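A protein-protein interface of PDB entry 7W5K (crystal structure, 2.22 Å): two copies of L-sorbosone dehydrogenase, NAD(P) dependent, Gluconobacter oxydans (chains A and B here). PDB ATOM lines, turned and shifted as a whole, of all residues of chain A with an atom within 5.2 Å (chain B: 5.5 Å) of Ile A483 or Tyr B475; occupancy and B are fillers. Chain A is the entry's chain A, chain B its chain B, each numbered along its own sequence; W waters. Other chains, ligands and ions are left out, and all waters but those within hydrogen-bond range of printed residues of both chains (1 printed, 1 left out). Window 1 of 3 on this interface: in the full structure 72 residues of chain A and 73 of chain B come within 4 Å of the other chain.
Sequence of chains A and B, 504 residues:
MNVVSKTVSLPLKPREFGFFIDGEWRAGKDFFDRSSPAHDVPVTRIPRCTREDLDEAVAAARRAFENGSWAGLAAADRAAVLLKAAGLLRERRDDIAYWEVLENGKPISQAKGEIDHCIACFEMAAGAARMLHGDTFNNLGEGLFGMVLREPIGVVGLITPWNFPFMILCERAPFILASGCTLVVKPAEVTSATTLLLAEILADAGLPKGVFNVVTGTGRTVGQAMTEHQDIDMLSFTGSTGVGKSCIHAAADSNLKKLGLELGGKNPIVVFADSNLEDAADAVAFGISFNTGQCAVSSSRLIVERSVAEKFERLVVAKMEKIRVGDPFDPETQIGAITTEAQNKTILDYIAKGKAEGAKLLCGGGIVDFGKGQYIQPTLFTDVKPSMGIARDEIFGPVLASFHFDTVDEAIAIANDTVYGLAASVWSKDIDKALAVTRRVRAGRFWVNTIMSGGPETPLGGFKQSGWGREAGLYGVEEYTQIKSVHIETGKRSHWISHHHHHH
The backbone carbonyl oxygen (O) of Pro B459 sits at hydrogen-bond distance from the side-chain hydroxyl (OG) of Ser A485 (2.4 Å).
N of Ser A485 lies within hydrogen-bond range of O of Gly B444 (2.8 Å).
The guanidinium group (NH2) of Arg B470 lies within hydrogen-bond range of the backbone carbonyl oxygen (O) of Ile A483 (2.7 Å).
The side-chain carboxylate of Asp A135 is in hydrogen-bond range of the side-chain hydroxyl of Tyr B475, 2.5 Å away.
The guanidinium group of Arg B470 sits at hydrogen-bond distance from the side-chain amide oxygen of Gln A482, at 3.0 Å.
NH1 of Arg A150 lies within hydrogen-bond range of OG1 of Thr A481, 3.0 Å away.
The backbone NH (N) of Arg B470 lies within hydrogen-bond range of the side-chain carboxylate (OE2) of Glu B479 (2.5 Å).
The backbone NH (N) of Leu A149 sits at hydrogen-bond distance from the backbone carbonyl oxygen (O) of Lys A484 (2.7 Å).
O of Asp A135 is in hydrogen-bond range of N of Val A148.
Among the printed residues, merely in contact across the chains: Val A148 with Pro B459 (3.4 Å), Val A148 with Tyr B475 (3.8 Å), Arg A150 with Tyr B475 (3.3 Å), Gln A482 with Phe B463 (3.3 Å), Ile A483 with Gly B444 (3.7 Å), Ile A483 with Pro B459 (3.5 Å), Ile A483 with Phe B463 (3.6 Å), Ile A483 with Tyr B475 (3.7 Å), Lys A484 with Ala B443 (3.0 Å), Lys A484 with Gly B444 (3.4 Å), Lys A484 with Phe B463 (3.98 Å) and Ser A485 with Thr B458 (3.6 Å).
Printed residues of chain B within 4 Å of Asp A135: Tyr B475 (2.5 Å).
Printed residues of chain B within 4 Å of Arg A150: Tyr B475 (3.3 Å).
Of chain B, only Gly B444, Pro B459, Phe B463, Arg B470 and Tyr B475 come within 4 Å of Ile A483.
Of the printed residues of chain A, Thr B458 touches Ser A485 (3.6 Å).
Of the printed residues of chain A, Pro B459 touches Val A148 (3.4 Å), Ile A483 (3.5 Å) and Ser A485 (2.4 Å).
Tyr B475 touches four residues of chain A.
The nearest residue of chain B that does not touch Ile A483 is Ala B443 (5.0 Å).
The nearest printed residue of chain A that does not touch Phe B463 is Leu A149 (6.4 Å).
Of the 17 printed residues of chain B, 7 touch a printed residue of chain A.
Hydrophobic or aromatic side chains of chain B within 4 Å of the printed part of chain A: Pro B459, Phe B463 and Tyr B475.
Of the 10 printed residues of chain A, 7 touch a printed residue of chain B.
Hydrophobic or aromatic side chains of chain A within 4 Å of the printed part of chain B: Val A148 and Ile A483.
Among the printed residues, no Asp or Glu carboxylate lies within 4 Å of a Lys or Arg side-chain nitrogen of the other chain.
No position is printed for both chains.
Of the 17 pairs that touch across the chains among the printed residues, none has its exchanged pair printed and touching as well.
Water W1 lies within hydrogen-bond range of OE1 of Gln A482 (2.7 Å), N of Ile A483 (2.8 Å) and NH2 of Arg B470 (3.3 Å).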
ATOM      1  N   GLY A 134      -4.833  31.066   0.443  1.00  0.00           N
ATOM      2  CA  GLY A 134      -5.569  30.751   1.645  1.00  0.00           C
ATOM      3  C   GLY A 134      -6.863  30.074   1.266  1.00  0.00           C
ATOM      4  O   GLY A 134      -6.918  29.367   0.256  1.00  0.00           O
ATOM      5  N   ASP A 135      -7.916  30.290   2.040  1.00  0.00           N
ATOM      6  CA  ASP A 135      -9.176  29.609   1.818  1.00  0.00           C
ATOM      7  C   ASP A 135     -10.309  30.604   1.680  1.00  0.00           C
ATOM      8  O   ASP A 135     -10.290  31.682   2.282  1.00  0.00           O
ATOM      9  CB  ASP A 135      -9.509  28.666   2.970  1.00  0.00           C
ATOM     10  CG  ASP A 135      -8.384  27.745   3.296  1.00  0.00           C
ATOM     11  OD1 ASP A 135      -7.841  27.121   2.364  1.00  0.00           O
ATOM     12  OD2 ASP A 135      -8.030  27.664   4.484  1.00  0.00           O
ATOM     13  N   VAL A 148      -9.766  32.907   4.403  1.00  0.00           N
ATOM     14  CA  VAL A 148      -8.495  32.866   5.090  1.00  0.00           C
ATOM     15  C   VAL A 148      -7.462  33.364   4.104  1.00  0.00           C
ATOM     16  O   VAL A 148      -7.313  32.795   3.017  1.00  0.00           O
ATOM     17  CB  VAL A 148      -8.153  31.456   5.580  1.00  0.00           C
ATOM     18  CG1 VAL A 148      -6.874  31.497   6.366  1.00  0.00           C
ATOM     19  CG2 VAL A 148      -9.278  30.944   6.428  1.00  0.00           C
ATOM     20  N   LEU A 149      -6.817  34.468   4.451  1.00  0.00           N
ATOM     21  CA  LEU A 149      -5.729  35.023   3.674  1.00  0.00           C
ATOM     22  C   LEU A 149      -4.396  34.542   4.224  1.00  0.00           C
ATOM     23  O   LEU A 149      -4.240  34.305   5.425  1.00  0.00           O
ATOM     24  CB  LEU A 149      -5.762  36.553   3.705  1.00  0.00           C
ATOM     25  CG  LEU A 149      -7.083  37.198   3.272  1.00  0.00           C
ATOM     26  CD1 LEU A 149      -6.954  38.717   3.145  1.00  0.00           C
ATOM     27  CD2 LEU A 149      -7.556  36.590   1.974  1.00  0.00           C
ATOM     28  N   ARG A 150      -3.438  34.385   3.328  1.00  0.00           N
ATOM     29  CA  ARG A 150      -2.047  34.260   3.707  1.00  0.00           C
ATOM     30  C   ARG A 150      -1.335  35.520   3.262  1.00  0.00           C
ATOM     31  O   ARG A 150      -1.659  36.097   2.217  1.00  0.00           O
ATOM     32  CB  ARG A 150      -1.390  33.028   3.087  1.00  0.00           C
ATOM     33  CG  ARG A 150      -1.849  31.745   3.745  1.00  0.00           C
ATOM     34  CD  ARG A 150      -1.013  30.560   3.309  1.00  0.00           C
ATOM     35  NE  ARG A 150      -1.438  29.353   4.002  1.00  0.00           N
ATOM     36  CZ  ARG A 150      -1.017  28.988   5.202  1.00  0.00           C
ATOM     37  NH1 ARG A 150      -0.124  29.702   5.867  1.00  0.00           N
ATOM     38  NH2 ARG A 150      -1.530  27.895   5.763  1.00  0.00           N
ATOM     39  N   THR A 481       4.345  32.969   6.150  1.00  0.00           N
ATOM     40  CA  THR A 481       3.166  33.766   5.938  1.00  0.00           C
ATOM     41  C   THR A 481       2.350  33.774   7.225  1.00  0.00           C
ATOM     42  O   THR A 481       2.452  32.863   8.055  1.00  0.00           O
ATOM     43  CB  THR A 481       2.356  33.213   4.759  1.00  0.00           C
ATOM     44  OG1 THR A 481       1.589  32.100   5.238  1.00  0.00           O
ATOM     45  N   GLN A 482       1.558  34.823   7.404  1.00  0.00           N
ATOM     46  CA  GLN A 482       0.592  34.846   8.481  1.00  0.00           C
ATOM     47  C   GLN A 482      -0.767  34.504   7.907  1.00  0.00           C
ATOM     48  O   GLN A 482      -1.074  34.855   6.767  1.00  0.00           O
ATOM     49  CB  GLN A 482       0.542  36.202   9.188  1.00  0.00           C
ATOM     50  CG  GLN A 482       1.661  36.406  10.187  1.00  0.00           C
ATOM     51  CD  GLN A 482       1.424  35.669  11.488  1.00  0.00           C
ATOM     52  OE1 GLN A 482       0.647  34.716  11.556  1.00  0.00           O
ATOM     53  NE2 GLN A 482       2.080  36.116  12.529  1.00  0.00           N
ATOM     54  N   ILE A 483      -1.540  33.763   8.683  1.00  0.00           N
ATOM     55  CA  ILE A 483      -2.886  33.373   8.320  1.00  0.00           C
ATOM     56  C   ILE A 483      -3.841  34.413   8.885  1.00  0.00           C
ATOM     57  O   ILE A 483      -3.796  34.713  10.086  1.00  0.00           O
ATOM     58  CB  ILE A 483      -3.200  31.976   8.864  1.00  0.00           C
ATOM     59  CG1 ILE A 483      -2.579  30.916   7.957  1.00  0.00           C
ATOM     60  CG2 ILE A 483      -4.708  31.793   9.077  1.00  0.00           C
ATOM     61  CD1 ILE A 483      -2.164  29.687   8.706  1.00  0.00           C
ATOM     62  N   LYS A 484      -4.687  34.980   8.021  1.00  0.00           N
ATOM     63  CA  LYS A 484      -5.637  36.016   8.412  1.00  0.00           C
ATOM     64  C   LYS A 484      -7.043  35.548   8.056  1.00  0.00           C
ATOM     65  O   LYS A 484      -7.396  35.437   6.877  1.00  0.00           O
ATOM     66  CB  LYS A 484      -5.315  37.357   7.755  1.00  0.00           C
ATOM     67  CG  LYS A 484      -6.369  38.429   7.984  1.00  0.00           C
ATOM     68  CD  LYS A 484      -6.012  39.712   7.242  1.00  0.00           C
ATOM     69  CE  LYS A 484      -4.884  40.446   7.940  1.00  0.00           C
ATOM     70  NZ  LYS A 484      -4.141  41.423   7.037  1.00  0.00           N
ATOM     71  N   SER A 485      -7.830  35.246   9.071  1.00  0.00           N
ATOM     72  CA  SER A 485      -9.222  34.915   8.855  1.00  0.00           C
ATOM     73  C   SER A 485     -10.008  36.191   8.646  1.00  0.00           C
ATOM     74  O   SER A 485      -9.791  37.194   9.325  1.00  0.00           O
ATOM     75  CB  SER A 485      -9.771  34.149  10.046  1.00  0.00           C
ATOM     76  OG  SER A 485      -9.328  32.805   9.946  1.00  0.00           O
ATOM     77  N   ALA B 443      -3.614  41.663  11.546  1.00  0.00           N
ATOM     78  CA  ALA B 443      -4.445  40.999  12.535  1.00  0.00           C
ATOM     79  C   ALA B 443      -4.824  39.630  12.002  1.00  0.00           C
ATOM     80  O   ALA B 443      -5.130  39.488  10.818  1.00  0.00           O
ATOM     81  CB  ALA B 443      -5.708  41.793  12.845  1.00  0.00           C
ATOM     82  N   GLY B 444      -4.833  38.630  12.885  1.00  0.00           N
ATOM     83  CA  GLY B 444      -5.122  37.272  12.457  1.00  0.00           C
ATOM     84  C   GLY B 444      -6.591  36.973  12.288  1.00  0.00           C
ATOM     85  O   GLY B 444      -6.947  36.015  11.594  1.00  0.00           O
ATOM     86  N   THR B 458     -12.972  28.424  10.470  1.00  0.00           N
ATOM     87  CA  THR B 458     -11.821  29.215  10.109  1.00  0.00           C
ATOM     88  C   THR B 458     -10.776  29.184  11.225  1.00  0.00           C
ATOM     89  O   THR B 458     -11.118  29.095  12.409  1.00  0.00           O
ATOM     90  CB  THR B 458     -12.237  30.663   9.819  1.00  0.00           C
ATOM     91  OG1 THR B 458     -13.060  31.138  10.879  1.00  0.00           O
ATOM     92  CG2 THR B 458     -13.038  30.743   8.520  1.00  0.00           C
ATOM     93  N   PRO B 459      -9.495  29.244  10.875  1.00  0.00           N
ATOM     94  CA  PRO B 459      -8.457  29.311  11.905  1.00  0.00           C
ATOM     95  C   PRO B 459      -8.503  30.648  12.614  1.00  0.00           C
ATOM     96  O   PRO B 459      -8.932  31.663  12.065  1.00  0.00           O
ATOM     97  CB  PRO B 459      -7.156  29.163  11.108  1.00  0.00           C
ATOM     98  CG  PRO B 459      -7.478  29.845   9.825  1.00  0.00           C
ATOM     99  CD  PRO B 459      -8.938  29.486   9.536  1.00  0.00           C
ATOM    100  N   GLY B 461      -6.122  33.159  15.364  1.00  0.00           N
ATOM    101  CA  GLY B 461      -4.824  33.382  15.953  1.00  0.00           C
ATOM    102  C   GLY B 461      -4.414  34.800  15.646  1.00  0.00           C
ATOM    103  O   GLY B 461      -5.158  35.570  15.039  1.00  0.00           O
ATOM    104  N   PHE B 463      -1.247  37.869  14.766  1.00  0.00           N
ATOM    105  CA  PHE B 463       0.060  38.304  14.313  1.00  0.00           C
ATOM    106  C   PHE B 463       0.855  38.777  15.508  1.00  0.00           C
ATOM    107  O   PHE B 463       0.325  38.936  16.612  1.00  0.00           O
ATOM    108  CB  PHE B 463      -0.037  39.465  13.322  1.00  0.00           C
ATOM    109  CG  PHE B 463      -0.623  39.103  11.981  1.00  0.00           C
ATOM    110  CD1 PHE B 463      -1.703  38.231  11.871  1.00  0.00           C
ATOM    111  CD2 PHE B 463      -0.118  39.683  10.839  1.00  0.00           C
ATOM    112  CE1 PHE B 463      -2.258  37.941  10.628  1.00  0.00           C
ATOM    113  CE2 PHE B 463      -0.661  39.411   9.600  1.00  0.00           C
ATOM    114  CZ  PHE B 463      -1.745  38.540   9.485  1.00  0.00           C
ATOM    115  N   ARG B 470      -2.219  28.822  14.820  1.00  0.00           N
ATOM    116  CA  ARG B 470      -3.633  29.056  14.638  1.00  0.00           C
ATOM    117  C   ARG B 470      -4.414  27.942  15.316  1.00  0.00           C
ATOM    118  O   ARG B 470      -3.919  26.824  15.473  1.00  0.00           O
ATOM    119  CB  ARG B 470      -4.004  29.101  13.141  1.00  0.00           C
ATOM    120  CG  ARG B 470      -3.524  30.334  12.406  1.00  0.00           C
ATOM    121  CD  ARG B 470      -4.060  31.575  13.076  1.00  0.00           C
ATOM    122  NE  ARG B 470      -3.589  32.806  12.455  1.00  0.00           N
ATOM    123  CZ  ARG B 470      -2.565  33.526  12.892  1.00  0.00           C
ATOM    124  NH1 ARG B 470      -1.854  33.150  13.945  1.00  0.00           N
ATOM    125  NH2 ARG B 470      -2.260  34.658  12.270  1.00  0.00           N
ATOM    126  N   GLU B 471      -5.648  28.258  15.699  1.00  0.00           N
ATOM    127  CA  GLU B 471      -6.543  27.331  16.368  1.00  0.00           C
ATOM    128  C   GLU B 471      -7.833  27.254  15.574  1.00  0.00           C
ATOM    129  O   GLU B 471      -8.124  28.126  14.750  1.00  0.00           O
ATOM    130  CB  GLU B 471      -6.854  27.746  17.814  1.00  0.00           C
ATOM    131  CG  GLU B 471      -5.627  28.078  18.628  1.00  0.00           C
ATOM    132  CD  GLU B 471      -4.763  26.870  18.895  1.00  0.00           C
ATOM    133  OE1 GLU B 471      -5.258  25.728  18.773  1.00  0.00           O
ATOM    134  OE2 GLU B 471      -3.580  27.063  19.240  1.00  0.00           O
ATOM    135  N   ALA B 472      -8.604  26.199  15.842  1.00  0.00           N
ATOM    136  CA  ALA B 472      -9.840  25.926  15.122  1.00  0.00           C
ATOM    137  C   ALA B 472      -9.612  25.754  13.625  1.00  0.00           C
ATOM    138  O   ALA B 472      -8.477  25.803  13.147  1.00  0.00           O
ATOM    139  CB  ALA B 472     -10.867  27.026  15.385  1.00  0.00           C
ATOM    140  N   GLY B 473     -10.688  25.553  12.880  1.00  0.00           N
ATOM    141  CA  GLY B 473     -10.590  25.135  11.494  1.00  0.00           C
ATOM    142  C   GLY B 473      -9.867  23.791  11.400  1.00  0.00           C
ATOM    143  O   GLY B 473      -9.532  23.139  12.380  1.00  0.00           O
ATOM    144  N   LEU B 474      -9.620  23.388  10.160  1.00  0.00           N
ATOM    145  CA  LEU B 474      -8.687  22.290   9.966  1.00  0.00           C
ATOM    146  C   LEU B 474      -7.281  22.699  10.404  1.00  0.00           C
ATOM    147  O   LEU B 474      -6.547  21.876  10.965  1.00  0.00           O
ATOM    148  CB  LEU B 474      -8.726  21.823   8.514  1.00  0.00           C
ATOM    149  CG  LEU B 474      -7.900  20.589   8.128  1.00  0.00           C
ATOM    150  CD1 LEU B 474      -8.188  19.408   9.030  1.00  0.00           C
ATOM    151  CD2 LEU B 474      -8.204  20.237   6.675  1.00  0.00           C
ATOM    152  N   TYR B 475      -6.924  23.978  10.215  1.00  0.00           N
ATOM    153  CA  TYR B 475      -5.629  24.507  10.651  1.00  0.00           C
ATOM    154  C   TYR B 475      -5.339  24.153  12.096  1.00  0.00           C
ATOM    155  O   TYR B 475      -4.236  23.695  12.435  1.00  0.00           O
ATOM    156  CB  TYR B 475      -5.615  26.028  10.528  1.00  0.00           C
ATOM    157  CG  TYR B 475      -5.661  26.558   9.132  1.00  0.00           C
ATOM    158  CD1 TYR B 475      -6.877  26.800   8.493  1.00  0.00           C
ATOM    159  CD2 TYR B 475      -4.493  26.831   8.446  1.00  0.00           C
ATOM    160  CE1 TYR B 475      -6.918  27.306   7.187  1.00  0.00           C
ATOM    161  CE2 TYR B 475      -4.523  27.320   7.141  1.00  0.00           C
ATOM    162  CZ  TYR B 475      -5.730  27.552   6.518  1.00  0.00           C
ATOM    163  OH  TYR B 475      -5.720  28.040   5.224  1.00  0.00           O
ATOM    164  N   GLY B 476      -6.315  24.398  12.968  1.00  0.00           N
ATOM    165  CA  GLY B 476      -6.111  24.159  14.377  1.00  0.00           C
ATOM    166  C   GLY B 476      -5.868  22.708  14.688  1.00  0.00           C
ATOM    167  O   GLY B 476      -5.124  22.385  15.620  1.00  0.00           O
ATOM    168  N   VAL B 477      -6.502  21.808  13.931  1.00  0.00           N
ATOM    169  CA  VAL B 477      -6.187  20.393  14.078  1.00  0.00           C
ATOM    170  C   VAL B 477      -4.785  20.109  13.564  1.00  0.00           C
ATOM    171  O   VAL B 477      -3.990  19.420  14.220  1.00  0.00           O
ATOM    172  CB  VAL B 477      -7.239  19.546  13.351  1.00  0.00           C
ATOM    173  CG1 VAL B 477      -6.906  18.072  13.513  1.00  0.00           C
ATOM    174  CG2 VAL B 477      -8.607  19.888  13.877  1.00  0.00           C
ATOM    175  N   GLU B 478      -4.447  20.664  12.398  1.00  0.00           N
ATOM    176  CA  GLU B 478      -3.116  20.454  11.839  1.00  0.00           C
ATOM    177  C   GLU B 478      -2.043  21.049  12.737  1.00  0.00           C
ATOM    178  O   GLU B 478      -0.916  20.548  12.769  1.00  0.00           O
ATOM    179  CB  GLU B 478      -3.026  21.073  10.445  1.00  0.00           C
ATOM    180  CG  GLU B 478      -3.971  20.480   9.419  1.00  0.00           C
ATOM    181  CD  GLU B 478      -4.041  21.339   8.172  1.00  0.00           C
ATOM    182  OE1 GLU B 478      -3.763  22.555   8.284  1.00  0.00           O
ATOM    183  OE2 GLU B 478      -4.375  20.810   7.083  1.00  0.00           O
ATOM    184  N   GLU B 479      -2.387  22.100  13.489  1.00  0.00           N
ATOM    185  CA  GLU B 479      -1.407  22.766  14.336  1.00  0.00           C
ATOM    186  C   GLU B 479      -0.815  21.816  15.363  1.00  0.00           C
ATOM    187  O   GLU B 479       0.331  21.996  15.788  1.00  0.00           O
ATOM    188  CB  GLU B 479      -2.052  23.970  15.033  1.00  0.00           C
ATOM    189  CG  GLU B 479      -1.086  25.131  15.263  1.00  0.00           C
ATOM    190  CD  GLU B 479      -0.629  25.798  13.966  1.00  0.00           C
ATOM    191  OE1 GLU B 479       0.058  25.162  13.126  1.00  0.00           O
ATOM    192  OE2 GLU B 479      -0.954  26.974  13.782  1.00  0.00           O
ATOM    193  N   TYR B 480      -1.583  20.812  15.776  1.00  0.00           N
ATOM    194  CA  TYR B 480      -1.171  19.844  16.780  1.00  0.00           C
ATOM    195  C   TYR B 480      -0.747  18.522  16.165  1.00  0.00           C
ATOM    196  O   TYR B 480      -0.725  17.495  16.845  1.00  0.00           O
ATOM    197  CB  TYR B 480      -2.295  19.664  17.790  1.00  0.00           C
ATOM    198  CG  TYR B 480      -2.568  20.981  18.469  1.00  0.00           C
ATOM    199  CD1 TYR B 480      -3.421  21.911  17.903  1.00  0.00           C
ATOM    200  CD2 TYR B 480      -1.928  21.310  19.653  1.00  0.00           C
ATOM    201  CE1 TYR B 480      -3.646  23.132  18.505  1.00  0.00           C
ATOM    202  CE2 TYR B 480      -2.152  22.521  20.263  1.00  0.00           C
ATOM    203  CZ  TYR B 480      -3.006  23.428  19.677  1.00  0.00           C
ATOM    204  OH  TYR B 480      -3.218  24.633  20.284  1.00  0.00           O
HETATM  205  O   HOH W   1      -0.383  32.346  10.792  1.00  0.00           O
